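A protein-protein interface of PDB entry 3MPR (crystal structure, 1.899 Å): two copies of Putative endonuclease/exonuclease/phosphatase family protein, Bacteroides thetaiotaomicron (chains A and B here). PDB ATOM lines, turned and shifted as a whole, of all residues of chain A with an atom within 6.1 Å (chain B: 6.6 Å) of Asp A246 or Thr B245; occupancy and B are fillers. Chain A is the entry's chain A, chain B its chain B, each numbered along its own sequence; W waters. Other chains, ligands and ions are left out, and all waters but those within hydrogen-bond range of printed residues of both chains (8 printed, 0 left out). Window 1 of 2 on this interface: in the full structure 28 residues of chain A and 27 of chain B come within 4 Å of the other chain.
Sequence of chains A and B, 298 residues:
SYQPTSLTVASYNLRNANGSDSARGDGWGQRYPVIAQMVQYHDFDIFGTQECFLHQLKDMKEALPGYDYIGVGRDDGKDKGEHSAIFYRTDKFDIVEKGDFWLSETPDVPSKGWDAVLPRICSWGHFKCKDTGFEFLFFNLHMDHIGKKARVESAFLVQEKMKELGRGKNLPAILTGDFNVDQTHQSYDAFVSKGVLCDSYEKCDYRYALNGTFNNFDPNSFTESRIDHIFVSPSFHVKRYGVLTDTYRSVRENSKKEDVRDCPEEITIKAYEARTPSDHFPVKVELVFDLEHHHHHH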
ATOM      1  N   MET A  38       0.320   3.724 -15.667  1.00  0.00           N
ATOM      2  CA  MET A  38       0.457   2.962 -16.919  1.00  0.00           C
ATOM      3  C   MET A  38      -0.023   1.521 -16.768  1.00  0.00           C
ATOM      4  O   MET A  38      -0.701   0.986 -17.647  1.00  0.00           O
ATOM      5  CB  MET A  38       1.898   2.958 -17.409  1.00  0.00           C
ATOM      6  CG  MET A  38       2.429   4.330 -17.774  1.00  0.00           C
ATOM      7  SD  MET A  38       4.190   4.200 -18.605  1.00  0.00           S
ATOM      8  CE  MET A  38       3.678   3.212 -20.191  1.00  0.00           C
ATOM      9  N   TYR A  41      -3.858   1.803 -16.637  1.00  0.00           N
ATOM     10  CA  TYR A  41      -4.456   2.211 -17.909  1.00  0.00           C
ATOM     11  C   TYR A  41      -4.277   1.165 -19.003  1.00  0.00           C
ATOM     12  O   TYR A  41      -5.175   0.946 -19.825  1.00  0.00           O
ATOM     13  CB  TYR A  41      -3.886   3.550 -18.380  1.00  0.00           C
ATOM     14  CG  TYR A  41      -4.622   4.066 -19.597  1.00  0.00           C
ATOM     15  CD1 TYR A  41      -5.832   4.717 -19.463  1.00  0.00           C
ATOM     16  CD2 TYR A  41      -4.127   3.854 -20.882  1.00  0.00           C
ATOM     17  CE1 TYR A  41      -6.520   5.183 -20.560  1.00  0.00           C
ATOM     18  CE2 TYR A  41      -4.818   4.310 -21.991  1.00  0.00           C
ATOM     19  CZ  TYR A  41      -6.007   4.971 -21.824  1.00  0.00           C
ATOM     20  OH  TYR A  41      -6.711   5.413 -22.921  1.00  0.00           O
ATOM     21  N   HIS A  42      -3.113   0.526 -19.016  1.00  0.00           N
ATOM     22  CA  HIS A  42      -2.796  -0.455 -20.052  1.00  0.00           C
ATOM     23  C   HIS A  42      -3.170  -1.884 -19.662  1.00  0.00           C
ATOM     24  O   HIS A  42      -2.817  -2.833 -20.351  1.00  0.00           O
ATOM     25  CB  HIS A  42      -1.329  -0.342 -20.472  1.00  0.00           C
ATOM     26  CG  HIS A  42      -1.037   0.891 -21.275  1.00  0.00           C
ATOM     27  ND1 HIS A  42      -0.418   2.003 -20.746  1.00  0.00           N
ATOM     28  CD2 HIS A  42      -1.300   1.187 -22.571  1.00  0.00           C
ATOM     29  CE1 HIS A  42      -0.313   2.932 -21.682  1.00  0.00           C
ATOM     30  NE2 HIS A  42      -0.834   2.458 -22.800  1.00  0.00           N
ATOM     31  N   VAL A 243       5.455  -1.747 -27.425  1.00  0.00           N
ATOM     32  CA  VAL A 243       6.332  -0.999 -26.538  1.00  0.00           C
ATOM     33  C   VAL A 243       5.640   0.322 -26.223  1.00  0.00           C
ATOM     34  O   VAL A 243       5.278   1.082 -27.130  1.00  0.00           O
ATOM     35  CB  VAL A 243       7.690  -0.735 -27.211  1.00  0.00           C
ATOM     36  CG1 VAL A 243       8.545   0.154 -26.353  1.00  0.00           C
ATOM     37  CG2 VAL A 243       8.405  -2.053 -27.491  1.00  0.00           C
ATOM     38  N   LEU A 244       5.448   0.603 -24.939  1.00  0.00           N
ATOM     39  CA  LEU A 244       4.686   1.780 -24.535  1.00  0.00           C
ATOM     40  C   LEU A 244       5.638   2.942 -24.243  1.00  0.00           C
ATOM     41  O   LEU A 244       6.417   2.906 -23.292  1.00  0.00           O
ATOM     42  CB  LEU A 244       3.815   1.444 -23.319  1.00  0.00           C
ATOM     43  CG  LEU A 244       3.033   0.123 -23.522  1.00  0.00           C
ATOM     44  CD1 LEU A 244       2.167  -0.225 -22.315  1.00  0.00           C
ATOM     45  CD2 LEU A 244       2.182   0.177 -24.788  1.00  0.00           C
ATOM     46  N   THR A 245       5.560   3.972 -25.077  1.00  0.00           N
ATOM     47  CA  THR A 245       6.493   5.096 -25.038  1.00  0.00           C
ATOM     48  C   THR A 245       5.960   6.291 -24.240  1.00  0.00           C
ATOM     49  O   THR A 245       6.519   7.393 -24.315  1.00  0.00           O
ATOM     50  CB  THR A 245       6.833   5.559 -26.485  1.00  0.00           C
ATOM     51  OG1 THR A 245       5.640   5.963 -27.170  1.00  0.00           O
ATOM     52  CG2 THR A 245       7.484   4.412 -27.264  1.00  0.00           C
ATOM     53  N   ASP A 246       4.900   6.062 -23.464  1.00  0.00           N
ATOM     54  CA  ASP A 246       4.205   7.140 -22.762  1.00  0.00           C
ATOM     55  C   ASP A 246       5.230   7.952 -21.980  1.00  0.00           C
ATOM     56  O   ASP A 246       6.149   7.380 -21.389  1.00  0.00           O
ATOM     57  CB  ASP A 246       3.181   6.589 -21.758  1.00  0.00           C
ATOM     58  CG  ASP A 246       2.178   5.624 -22.368  1.00  0.00           C
ATOM     59  OD1 ASP A 246       2.526   4.868 -23.301  1.00  0.00           O
ATOM     60  OD2 ASP A 246       1.034   5.589 -21.850  1.00  0.00           O
ATOM     61  N   THR A 247       5.081   9.275 -21.974  1.00  0.00           N
ATOM     62  CA  THR A 247       5.954  10.125 -21.161  1.00  0.00           C
ATOM     63  C   THR A 247       5.166  11.129 -20.330  1.00  0.00           C
ATOM     64  O   THR A 247       4.085  11.583 -20.732  1.00  0.00           O
ATOM     65  CB  THR A 247       6.952  10.937 -22.040  1.00  0.00           C
ATOM     66  OG1 THR A 247       6.239  11.556 -23.115  1.00  0.00           O
ATOM     67  CG2 THR A 247       8.033  10.043 -22.613  1.00  0.00           C
ATOM     68  N   TYR A 248       5.720  11.489 -19.180  1.00  0.00           N
ATOM     69  CA  TYR A 248       5.156  12.558 -18.372  1.00  0.00           C
ATOM     70  C   TYR A 248       6.011  13.818 -18.544  1.00  0.00           C
ATOM     71  O   TYR A 248       6.900  13.853 -19.400  1.00  0.00           O
ATOM     72  CB  TYR A 248       5.009  12.126 -16.899  1.00  0.00           C
ATOM     73  CG  TYR A 248       6.299  11.987 -16.091  1.00  0.00           C
ATOM     74  CD1 TYR A 248       6.673  12.971 -15.192  1.00  0.00           C
ATOM     75  CD2 TYR A 248       7.103  10.857 -16.189  1.00  0.00           C
ATOM     76  CE1 TYR A 248       7.819  12.857 -14.429  1.00  0.00           C
ATOM     77  CE2 TYR A 248       8.271  10.727 -15.418  1.00  0.00           C
ATOM     78  CZ  TYR A 248       8.614  11.742 -14.538  1.00  0.00           C
ATOM     79  OH  TYR A 248       9.755  11.674 -13.768  1.00  0.00           O
ATOM     80  N   ARG A 249       5.731  14.859 -17.766  1.00  0.00           N
ATOM     81  CA  ARG A 249       6.464  16.114 -17.926  1.00  0.00           C
ATOM     82  C   ARG A 249       6.888  16.633 -16.573  1.00  0.00           C
ATOM     83  O   ARG A 249       6.174  16.451 -15.588  1.00  0.00           O
ATOM     84  CB  ARG A 249       5.611  17.183 -18.615  1.00  0.00           C
ATOM     85  CG  ARG A 249       5.126  16.824 -20.029  1.00  0.00           C
ATOM     86  CD  ARG A 249       6.224  16.905 -21.105  1.00  0.00           C
ATOM     87  NE  ARG A 249       5.646  16.592 -22.413  1.00  0.00           N
ATOM     88  CZ  ARG A 249       5.512  15.359 -22.891  1.00  0.00           C
ATOM     89  NH1 ARG A 249       5.961  14.325 -22.183  1.00  0.00           N
ATOM     90  NH2 ARG A 249       4.942  15.161 -24.079  1.00  0.00           N
ATOM     91  N   ARG A 275       9.864  13.335 -19.649  1.00  0.00           N
ATOM     92  CA  ARG A 275      10.543  12.412 -18.743  1.00  0.00           C
ATOM     93  C   ARG A 275       9.985  11.028 -19.016  1.00  0.00           C
ATOM     94  O   ARG A 275       8.783  10.889 -19.239  1.00  0.00           O
ATOM     95  CB  ARG A 275      10.200  12.757 -17.286  1.00  0.00           C
ATOM     96  CG  ARG A 275      10.764  14.068 -16.777  1.00  0.00           C
ATOM     97  CD  ARG A 275      12.217  13.889 -16.387  1.00  0.00           C
ATOM     98  NE  ARG A 275      12.809  15.136 -15.905  1.00  0.00           N
ATOM     99  CZ  ARG A 275      14.090  15.261 -15.570  1.00  0.00           C
ATOM    100  NH1 ARG A 275      14.906  14.216 -15.662  1.00  0.00           N
ATOM    101  NH2 ARG A 275      14.555  16.431 -15.148  1.00  0.00           N
ATOM    102  N   THR A 276      10.832  10.004 -18.984  1.00  0.00           N
ATOM    103  CA  THR A 276      10.334   8.643 -19.147  1.00  0.00           C
ATOM    104  C   THR A 276      10.056   8.075 -17.750  1.00  0.00           C
ATOM    105  O   THR A 276      10.810   8.337 -16.817  1.00  0.00           O
ATOM    106  CB  THR A 276      11.330   7.757 -19.908  1.00  0.00           C
ATOM    107  OG1 THR A 276      12.592   7.754 -19.219  1.00  0.00           O
ATOM    108  CG2 THR A 276      11.518   8.272 -21.326  1.00  0.00           C
ATOM    109  N   PRO A 277       8.953   7.329 -17.598  1.00  0.00           N
ATOM    110  CA  PRO A 277       8.575   6.799 -16.280  1.00  0.00           C
ATOM    111  C   PRO A 277       9.640   5.853 -15.717  1.00  0.00           C
ATOM    112  O   PRO A 277       9.793   5.782 -14.507  1.00  0.00           O
ATOM    113  CB  PRO A 277       7.269   6.055 -16.564  1.00  0.00           C
ATOM    114  CG  PRO A 277       6.690   6.780 -17.757  1.00  0.00           C
ATOM    115  CD  PRO A 277       7.886   7.148 -18.597  1.00  0.00           C
ATOM    116  N   PHE A 281      11.323   1.102 -21.484  1.00  0.00           N
ATOM    117  CA  PHE A 281       9.898   1.123 -21.800  1.00  0.00           C
ATOM    118  C   PHE A 281       9.294  -0.219 -21.418  1.00  0.00           C
ATOM    119  O   PHE A 281       9.941  -1.239 -21.589  1.00  0.00           O
ATOM    120  CB  PHE A 281       9.682   1.349 -23.290  1.00  0.00           C
ATOM    121  CG  PHE A 281      10.170   2.685 -23.772  1.00  0.00           C
ATOM    122  CD1 PHE A 281       9.709   3.850 -23.189  1.00  0.00           C
ATOM    123  CD2 PHE A 281      11.081   2.775 -24.808  1.00  0.00           C
ATOM    124  CE1 PHE A 281      10.151   5.080 -23.622  1.00  0.00           C
ATOM    125  CE2 PHE A 281      11.530   4.011 -25.244  1.00  0.00           C
ATOM    126  CZ  PHE A 281      11.064   5.158 -24.645  1.00  0.00           C
ATOM    127  N   MET B  38      -1.416   3.725 -34.058  1.00  0.00           N
ATOM    128  CA  MET B  38      -2.045   4.072 -32.790  1.00  0.00           C
ATOM    129  C   MET B  38      -3.525   3.747 -32.779  1.00  0.00           C
ATOM    130  O   MET B  38      -4.055   3.238 -31.792  1.00  0.00           O
ATOM    131  CB  MET B  38      -1.848   5.561 -32.476  1.00  0.00           C
ATOM    132  CG  MET B  38      -0.425   5.891 -32.092  1.00  0.00           C
ATOM    133  SD  MET B  38      -0.308   7.775 -31.614  1.00  0.00           S
ATOM    134  CE  MET B  38      -1.205   7.668 -29.877  1.00  0.00           C
ATOM    135  N   HIS B  42      -4.447   0.956 -30.083  1.00  0.00           N
ATOM    136  CA  HIS B  42      -5.252   1.482 -28.990  1.00  0.00           C
ATOM    137  C   HIS B  42      -6.737   1.178 -29.165  1.00  0.00           C
ATOM    138  O   HIS B  42      -7.556   1.611 -28.370  1.00  0.00           O
ATOM    139  CB  HIS B  42      -4.978   2.979 -28.805  1.00  0.00           C
ATOM    140  CG  HIS B  42      -3.641   3.254 -28.199  1.00  0.00           C
ATOM    141  ND1 HIS B  42      -2.577   3.753 -28.924  1.00  0.00           N
ATOM    142  CD2 HIS B  42      -3.184   3.074 -26.937  1.00  0.00           C
ATOM    143  CE1 HIS B  42      -1.530   3.884 -28.129  1.00  0.00           C
ATOM    144  NE2 HIS B  42      -1.868   3.472 -26.921  1.00  0.00           N
ATOM    145  N   TYR B 208      -6.536   9.041 -17.004  1.00  0.00           N
ATOM    146  CA  TYR B 208      -5.113   8.958 -17.308  1.00  0.00           C
ATOM    147  C   TYR B 208      -4.767  10.185 -18.139  1.00  0.00           C
ATOM    148  O   TYR B 208      -5.035  10.231 -19.341  1.00  0.00           O
ATOM    149  CB  TYR B 208      -4.836   7.677 -18.093  1.00  0.00           C
ATOM    150  CG  TYR B 208      -3.389   7.418 -18.458  1.00  0.00           C
ATOM    151  CD1 TYR B 208      -2.375   7.541 -17.516  1.00  0.00           C
ATOM    152  CD2 TYR B 208      -3.043   7.010 -19.747  1.00  0.00           C
ATOM    153  CE1 TYR B 208      -1.042   7.286 -17.852  1.00  0.00           C
ATOM    154  CE2 TYR B 208      -1.712   6.738 -20.088  1.00  0.00           C
ATOM    155  CZ  TYR B 208      -0.724   6.881 -19.134  1.00  0.00           C
ATOM    156  OH  TYR B 208       0.590   6.627 -19.449  1.00  0.00           O
ATOM    157  N   LEU B 210      -1.601  12.608 -18.537  1.00  0.00           N
ATOM    158  CA  LEU B 210      -0.240  13.089 -18.292  1.00  0.00           C
ATOM    159  C   LEU B 210       0.059  14.398 -19.027  1.00  0.00           C
ATOM    160  O   LEU B 210       1.176  14.921 -18.961  1.00  0.00           O
ATOM    161  CB  LEU B 210       0.781  12.032 -18.709  1.00  0.00           C
ATOM    162  CG  LEU B 210       0.665  10.656 -18.071  1.00  0.00           C
ATOM    163  CD1 LEU B 210       1.795   9.755 -18.579  1.00  0.00           C
ATOM    164  CD2 LEU B 210       0.715  10.780 -16.552  1.00  0.00           C
ATOM    165  N   ASN B 211      -0.935  14.903 -19.748  1.00  0.00           N
ATOM    166  CA  ASN B 211      -0.793  16.153 -20.474  1.00  0.00           C
ATOM    167  C   ASN B 211      -2.168  16.648 -20.909  1.00  0.00           C
ATOM    168  O   ASN B 211      -3.161  15.910 -20.816  1.00  0.00           O
ATOM    169  CB  ASN B 211       0.089  15.940 -21.709  1.00  0.00           C
ATOM    170  CG  ASN B 211       0.997  17.130 -22.004  1.00  0.00           C
ATOM    171  OD1 ASN B 211       0.574  18.289 -21.945  1.00  0.00           O
ATOM    172  ND2 ASN B 211       2.258  16.844 -22.313  1.00  0.00           N
ATOM    173  N   GLY B 212      -2.214  17.896 -21.374  1.00  0.00           N
ATOM    174  CA  GLY B 212      -3.377  18.441 -22.050  1.00  0.00           C
ATOM    175  C   GLY B 212      -3.385  17.893 -23.468  1.00  0.00           C
ATOM    176  O   GLY B 212      -2.657  16.948 -23.767  1.00  0.00           O
ATOM    177  N   VAL B 243      -5.241  10.418 -22.371  1.00  0.00           N
ATOM    178  CA  VAL B 243      -4.549  11.187 -23.393  1.00  0.00           C
ATOM    179  C   VAL B 243      -3.315  10.361 -23.767  1.00  0.00           C
ATOM    180  O   VAL B 243      -2.514  10.017 -22.900  1.00  0.00           O
ATOM    181  CB  VAL B 243      -4.112  12.554 -22.842  1.00  0.00           C
ATOM    182  CG1 VAL B 243      -3.255  13.300 -23.862  1.00  0.00           C
ATOM    183  CG2 VAL B 243      -5.334  13.373 -22.463  1.00  0.00           C
ATOM    184  N   LEU B 244      -3.169  10.020 -25.045  1.00  0.00           N
ATOM    185  CA  LEU B 244      -2.117   9.083 -25.452  1.00  0.00           C
ATOM    186  C   LEU B 244      -0.888   9.866 -25.915  1.00  0.00           C
ATOM    187  O   LEU B 244      -0.929  10.522 -26.952  1.00  0.00           O
ATOM    188  CB  LEU B 244      -2.623   8.173 -26.573  1.00  0.00           C
ATOM    189  CG  LEU B 244      -3.958   7.502 -26.259  1.00  0.00           C
ATOM    190  CD1 LEU B 244      -4.444   6.620 -27.432  1.00  0.00           C
ATOM    191  CD2 LEU B 244      -3.798   6.684 -24.981  1.00  0.00           C
ATOM    192  N   THR B 245       0.195   9.801 -25.140  1.00  0.00           N
ATOM    193  CA  THR B 245       1.374  10.625 -25.403  1.00  0.00           C
ATOM    194  C   THR B 245       2.428   9.899 -26.249  1.00  0.00           C
ATOM    195  O   THR B 245       3.560  10.383 -26.372  1.00  0.00           O
ATOM    196  CB  THR B 245       2.044  11.084 -24.079  1.00  0.00           C
ATOM    197  OG1 THR B 245       2.436   9.936 -23.320  1.00  0.00           O
ATOM    198  CG2 THR B 245       1.093  11.932 -23.239  1.00  0.00           C
ATOM    199  N   ASP B 246       2.069   8.749 -26.826  1.00  0.00           N
ATOM    200  CA  ASP B 246       3.014   7.978 -27.638  1.00  0.00           C
ATOM    201  C   ASP B 246       3.816   8.880 -28.572  1.00  0.00           C
ATOM    202  O   ASP B 246       3.255   9.777 -29.193  1.00  0.00           O
ATOM    203  CB  ASP B 246       2.312   6.935 -28.535  1.00  0.00           C
ATOM    204  CG  ASP B 246       1.341   6.028 -27.787  1.00  0.00           C
ATOM    205  OD1 ASP B 246       0.721   6.477 -26.801  1.00  0.00           O
ATOM    206  OD2 ASP B 246       1.156   4.873 -28.249  1.00  0.00           O
ATOM    207  N   THR B 247       5.115   8.614 -28.700  1.00  0.00           N
ATOM    208  CA  THR B 247       5.953   9.311 -29.671  1.00  0.00           C
ATOM    209  C   THR B 247       6.806   8.341 -30.497  1.00  0.00           C
ATOM    210  O   THR B 247       7.198   7.267 -30.018  1.00  0.00           O
ATOM    211  CB  THR B 247       6.906  10.317 -29.006  1.00  0.00           C
ATOM    212  OG1 THR B 247       7.584   9.669 -27.921  1.00  0.00           O
ATOM    213  CG2 THR B 247       6.154  11.539 -28.494  1.00  0.00           C
ATOM    214  N   ARG B 275       9.323  12.643 -31.869  1.00  0.00           N
ATOM    215  CA  ARG B 275       8.354  13.306 -32.730  1.00  0.00           C
ATOM    216  C   ARG B 275       6.956  12.925 -32.269  1.00  0.00           C
ATOM    217  O   ARG B 275       6.721  11.785 -31.890  1.00  0.00           O
ATOM    218  CB  ARG B 275       8.541  12.850 -34.177  1.00  0.00           C
ATOM    219  CG  ARG B 275       9.855  13.288 -34.811  1.00  0.00           C
ATOM    220  CD  ARG B 275       9.793  14.770 -35.211  1.00  0.00           C
ATOM    221  NE  ARG B 275      10.980  15.182 -35.961  1.00  0.00           N
ATOM    222  CZ  ARG B 275      11.133  16.378 -36.526  1.00  0.00           C
ATOM    223  NH1 ARG B 275      10.173  17.292 -36.426  1.00  0.00           N
ATOM    224  NH2 ARG B 275      12.247  16.655 -37.195  1.00  0.00           N
ATOM    225  N   THR B 276       6.020  13.868 -32.305  1.00  0.00           N
ATOM    226  CA  THR B 276       4.646  13.533 -31.969  1.00  0.00           C
ATOM    227  C   THR B 276       3.908  13.191 -33.260  1.00  0.00           C
ATOM    228  O   THR B 276       4.125  13.827 -34.289  1.00  0.00           O
ATOM    229  CB  THR B 276       3.954  14.669 -31.197  1.00  0.00           C
ATOM    230  OG1 THR B 276       3.997  15.871 -31.970  1.00  0.00           O
ATOM    231  CG2 THR B 276       4.680  14.917 -29.869  1.00  0.00           C
ATOM    232  N   PRO B 277       3.074  12.152 -33.222  1.00  0.00           N
ATOM    233  CA  PRO B 277       2.396  11.736 -34.457  1.00  0.00           C
ATOM    234  C   PRO B 277       1.504  12.832 -35.026  1.00  0.00           C
ATOM    235  O   PRO B 277       1.261  12.854 -36.222  1.00  0.00           O
ATOM    236  CB  PRO B 277       1.585  10.520 -34.017  1.00  0.00           C
ATOM    237  CG  PRO B 277       2.416   9.944 -32.829  1.00  0.00           C
ATOM    238  CD  PRO B 277       2.930  11.168 -32.129  1.00  0.00           C
ATOM    239  N   PHE B 281      -2.567  15.450 -29.083  1.00  0.00           N
ATOM    240  CA  PHE B 281      -2.586  14.050 -28.648  1.00  0.00           C
ATOM    241  C   PHE B 281      -4.009  13.545 -28.830  1.00  0.00           C
ATOM    242  O   PHE B 281      -4.967  14.328 -28.700  1.00  0.00           O
ATOM    243  CB  PHE B 281      -2.209  13.944 -27.165  1.00  0.00           C
ATOM    244  CG  PHE B 281      -0.793  14.336 -26.858  1.00  0.00           C
ATOM    245  CD1 PHE B 281       0.269  13.642 -27.409  1.00  0.00           C
ATOM    246  CD2 PHE B 281      -0.522  15.381 -25.978  1.00  0.00           C
ATOM    247  CE1 PHE B 281       1.585  13.984 -27.112  1.00  0.00           C
ATOM    248  CE2 PHE B 281       0.792  15.736 -25.678  1.00  0.00           C
ATOM    249  CZ  PHE B 281       1.848  15.036 -26.243  1.00  0.00           C
ATOM    250  N   PRO B 282      -4.169  12.244 -29.141  1.00  0.00           N
ATOM    251  CA  PRO B 282      -5.523  11.680 -29.162  1.00  0.00           C
ATOM    252  C   PRO B 282      -6.130  11.608 -27.758  1.00  0.00           C
ATOM    253  O   PRO B 282      -5.426  11.372 -26.768  1.00  0.00           O
ATOM    254  CB  PRO B 282      -5.313  10.244 -29.669  1.00  0.00           C
ATOM    255  CG  PRO B 282      -3.862  10.121 -30.010  1.00  0.00           C
ATOM    256  CD  PRO B 282      -3.135  11.208 -29.309  1.00  0.00           C
HETATM  257  O   HOH W   1       1.020   3.918 -25.364  1.00  0.00           O
HETATM  258  O   HOH W   2      -0.427   5.814 -24.445  1.00  0.00           O
HETATM  259  O   HOH W   3       0.173   8.461 -22.472  1.00  0.00           O
HETATM  260  O   HOH W   4       9.091   8.225 -25.256  1.00  0.00           O
HETATM  261  O   HOH W   5       4.767  12.974 -25.697  1.00  0.00           O
HETATM  262  O   HOH W   6       2.949  14.216 -20.962  1.00  0.00           O
HETATM  263  O   HOH W   7       6.104   9.702 -25.415  1.00  0.00           O
HETATM  264  O   HOH W   8       3.960   3.796 -27.510  1.00  0.00           O
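The side-chain hydroxyl (OH) of Tyr B208 lies within hydrogen-bond range of the side-chain carboxylate (OD2) of Asp A246, 2.7 Å away. ND2 of Asn B211 lies close to NE of Arg A249 (3.4 Å). N of Thr A247 is in hydrogen-bond range of OG1 of Thr B245. OG1 of Thr A245 lies within hydrogen-bond range of N of Thr B247 (3.1 Å).
O of Pro B282 is in hydrogen-bond range of N of Leu B244 (3.1 Å). The backbone carbonyl oxygen of Tyr B208 is in hydrogen-bond range of the backbone NH of Val B243 (3.0 Å). A ring nitrogen (ND1) of His A42 sits close to the backbone carbonyl oxygen (O) of Met A38, 3.3 Å away. OG1 of Thr A247 lies within hydrogen-bond range of NH1 of Arg A249, at 2.9 Å.
Among the printed residues, merely in contact across the chains: Met A38 with Tyr B208, Tyr A41 with Tyr B208, Tyr A41 with Leu B244, Thr A245 with Asp B246, Asp A246 with Thr B245, Thr A247 with Leu B210 and Arg A249 with Phe B281.
Of chain B, only Tyr B208 (2.7 Å) and Thr B245 (3.4 Å) come within 4 Å of Asp A246. Of the printed residues of chain A, Asn B211 touches Arg A249. Of the printed residues of chain A, Leu B244 touches Tyr A41 (3.8 Å). Thr B245 touches just these residues of chain A: Asp A246 (3.4 Å) and Thr A247 (3.0 Å). Printed residues of chain A within 4 Å of Thr B247: Thr A245 (3.1 Å). Of the printed residues of chain A, Phe B281 touches Arg A249 (3.8 Å). The nearest residue of chain A that does not touch Thr B245 is Thr A245 (4.7 Å). The nearest printed residue of chain B that does not touch Thr A247 is Thr B247 (5.3 Å).
Printed residues of chain A that touch a printed residue of chain B: Met A38, Tyr A41, Thr A245, Asp A246, Thr A247 and Arg A249. Hydrophobic or aromatic side chains of chain A within 4 Å of the printed part of chain B: Met A38 and Tyr A41. Hydrophobic or aromatic side chains of chain B that line the printed part of chain A: Tyr B208, Leu B210, Leu B244 and Phe B281. Among the printed residues, 11 pairs touch across the chains. Among the printed residues, no Asp or Glu carboxylate lies within 4 Å of a Lys or Arg side-chain nitrogen of the other chain.
Thr A245 touches Asp B246, and with the chains exchanged Asp A246 touches Thr B245. Thr A245 touches Thr B247, and with the chains exchanged Thr A247 touches Thr B245. 11 positions are printed for both chains.
Water W7 lies within hydrogen-bond range of O of Thr A245 (2.6 Å), O of Thr B245 (2.8 Å), OG1 of Thr B247 (2.9 Å) and OG1 of Thr A247 (3.0 Å). Water W2 bridges the side-chain carboxylate of Asp B246 (2.7 Å) and the side-chain carboxylate of Asp A246 (3.0 Å). Water W1 lies within hydrogen-bond range of the side-chain carboxylate of Asp A246, the side-chain carboxylate of Asp B246, a ring nitrogen (NE2) of His B42 and a ring nitrogen (NE2) of His A42. Water W6 lies within hydrogen-bond range of O of Leu B210 (2.8 Å), O of Thr A247 (2.9 Å), ND2 of Asn B211 (3.0 Å) and NH1 of Arg A249 (3.3 Å). Water W3 lies within hydrogen-bond range of the side-chain hydroxyl of Thr B245, the side-chain carboxylate of Asp A246 and the backbone carbonyl oxygen of Val B243. Water W4 bridges O of Thr A245 (2.9 Å) and OG1 of Thr B247 (3.4 Å).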
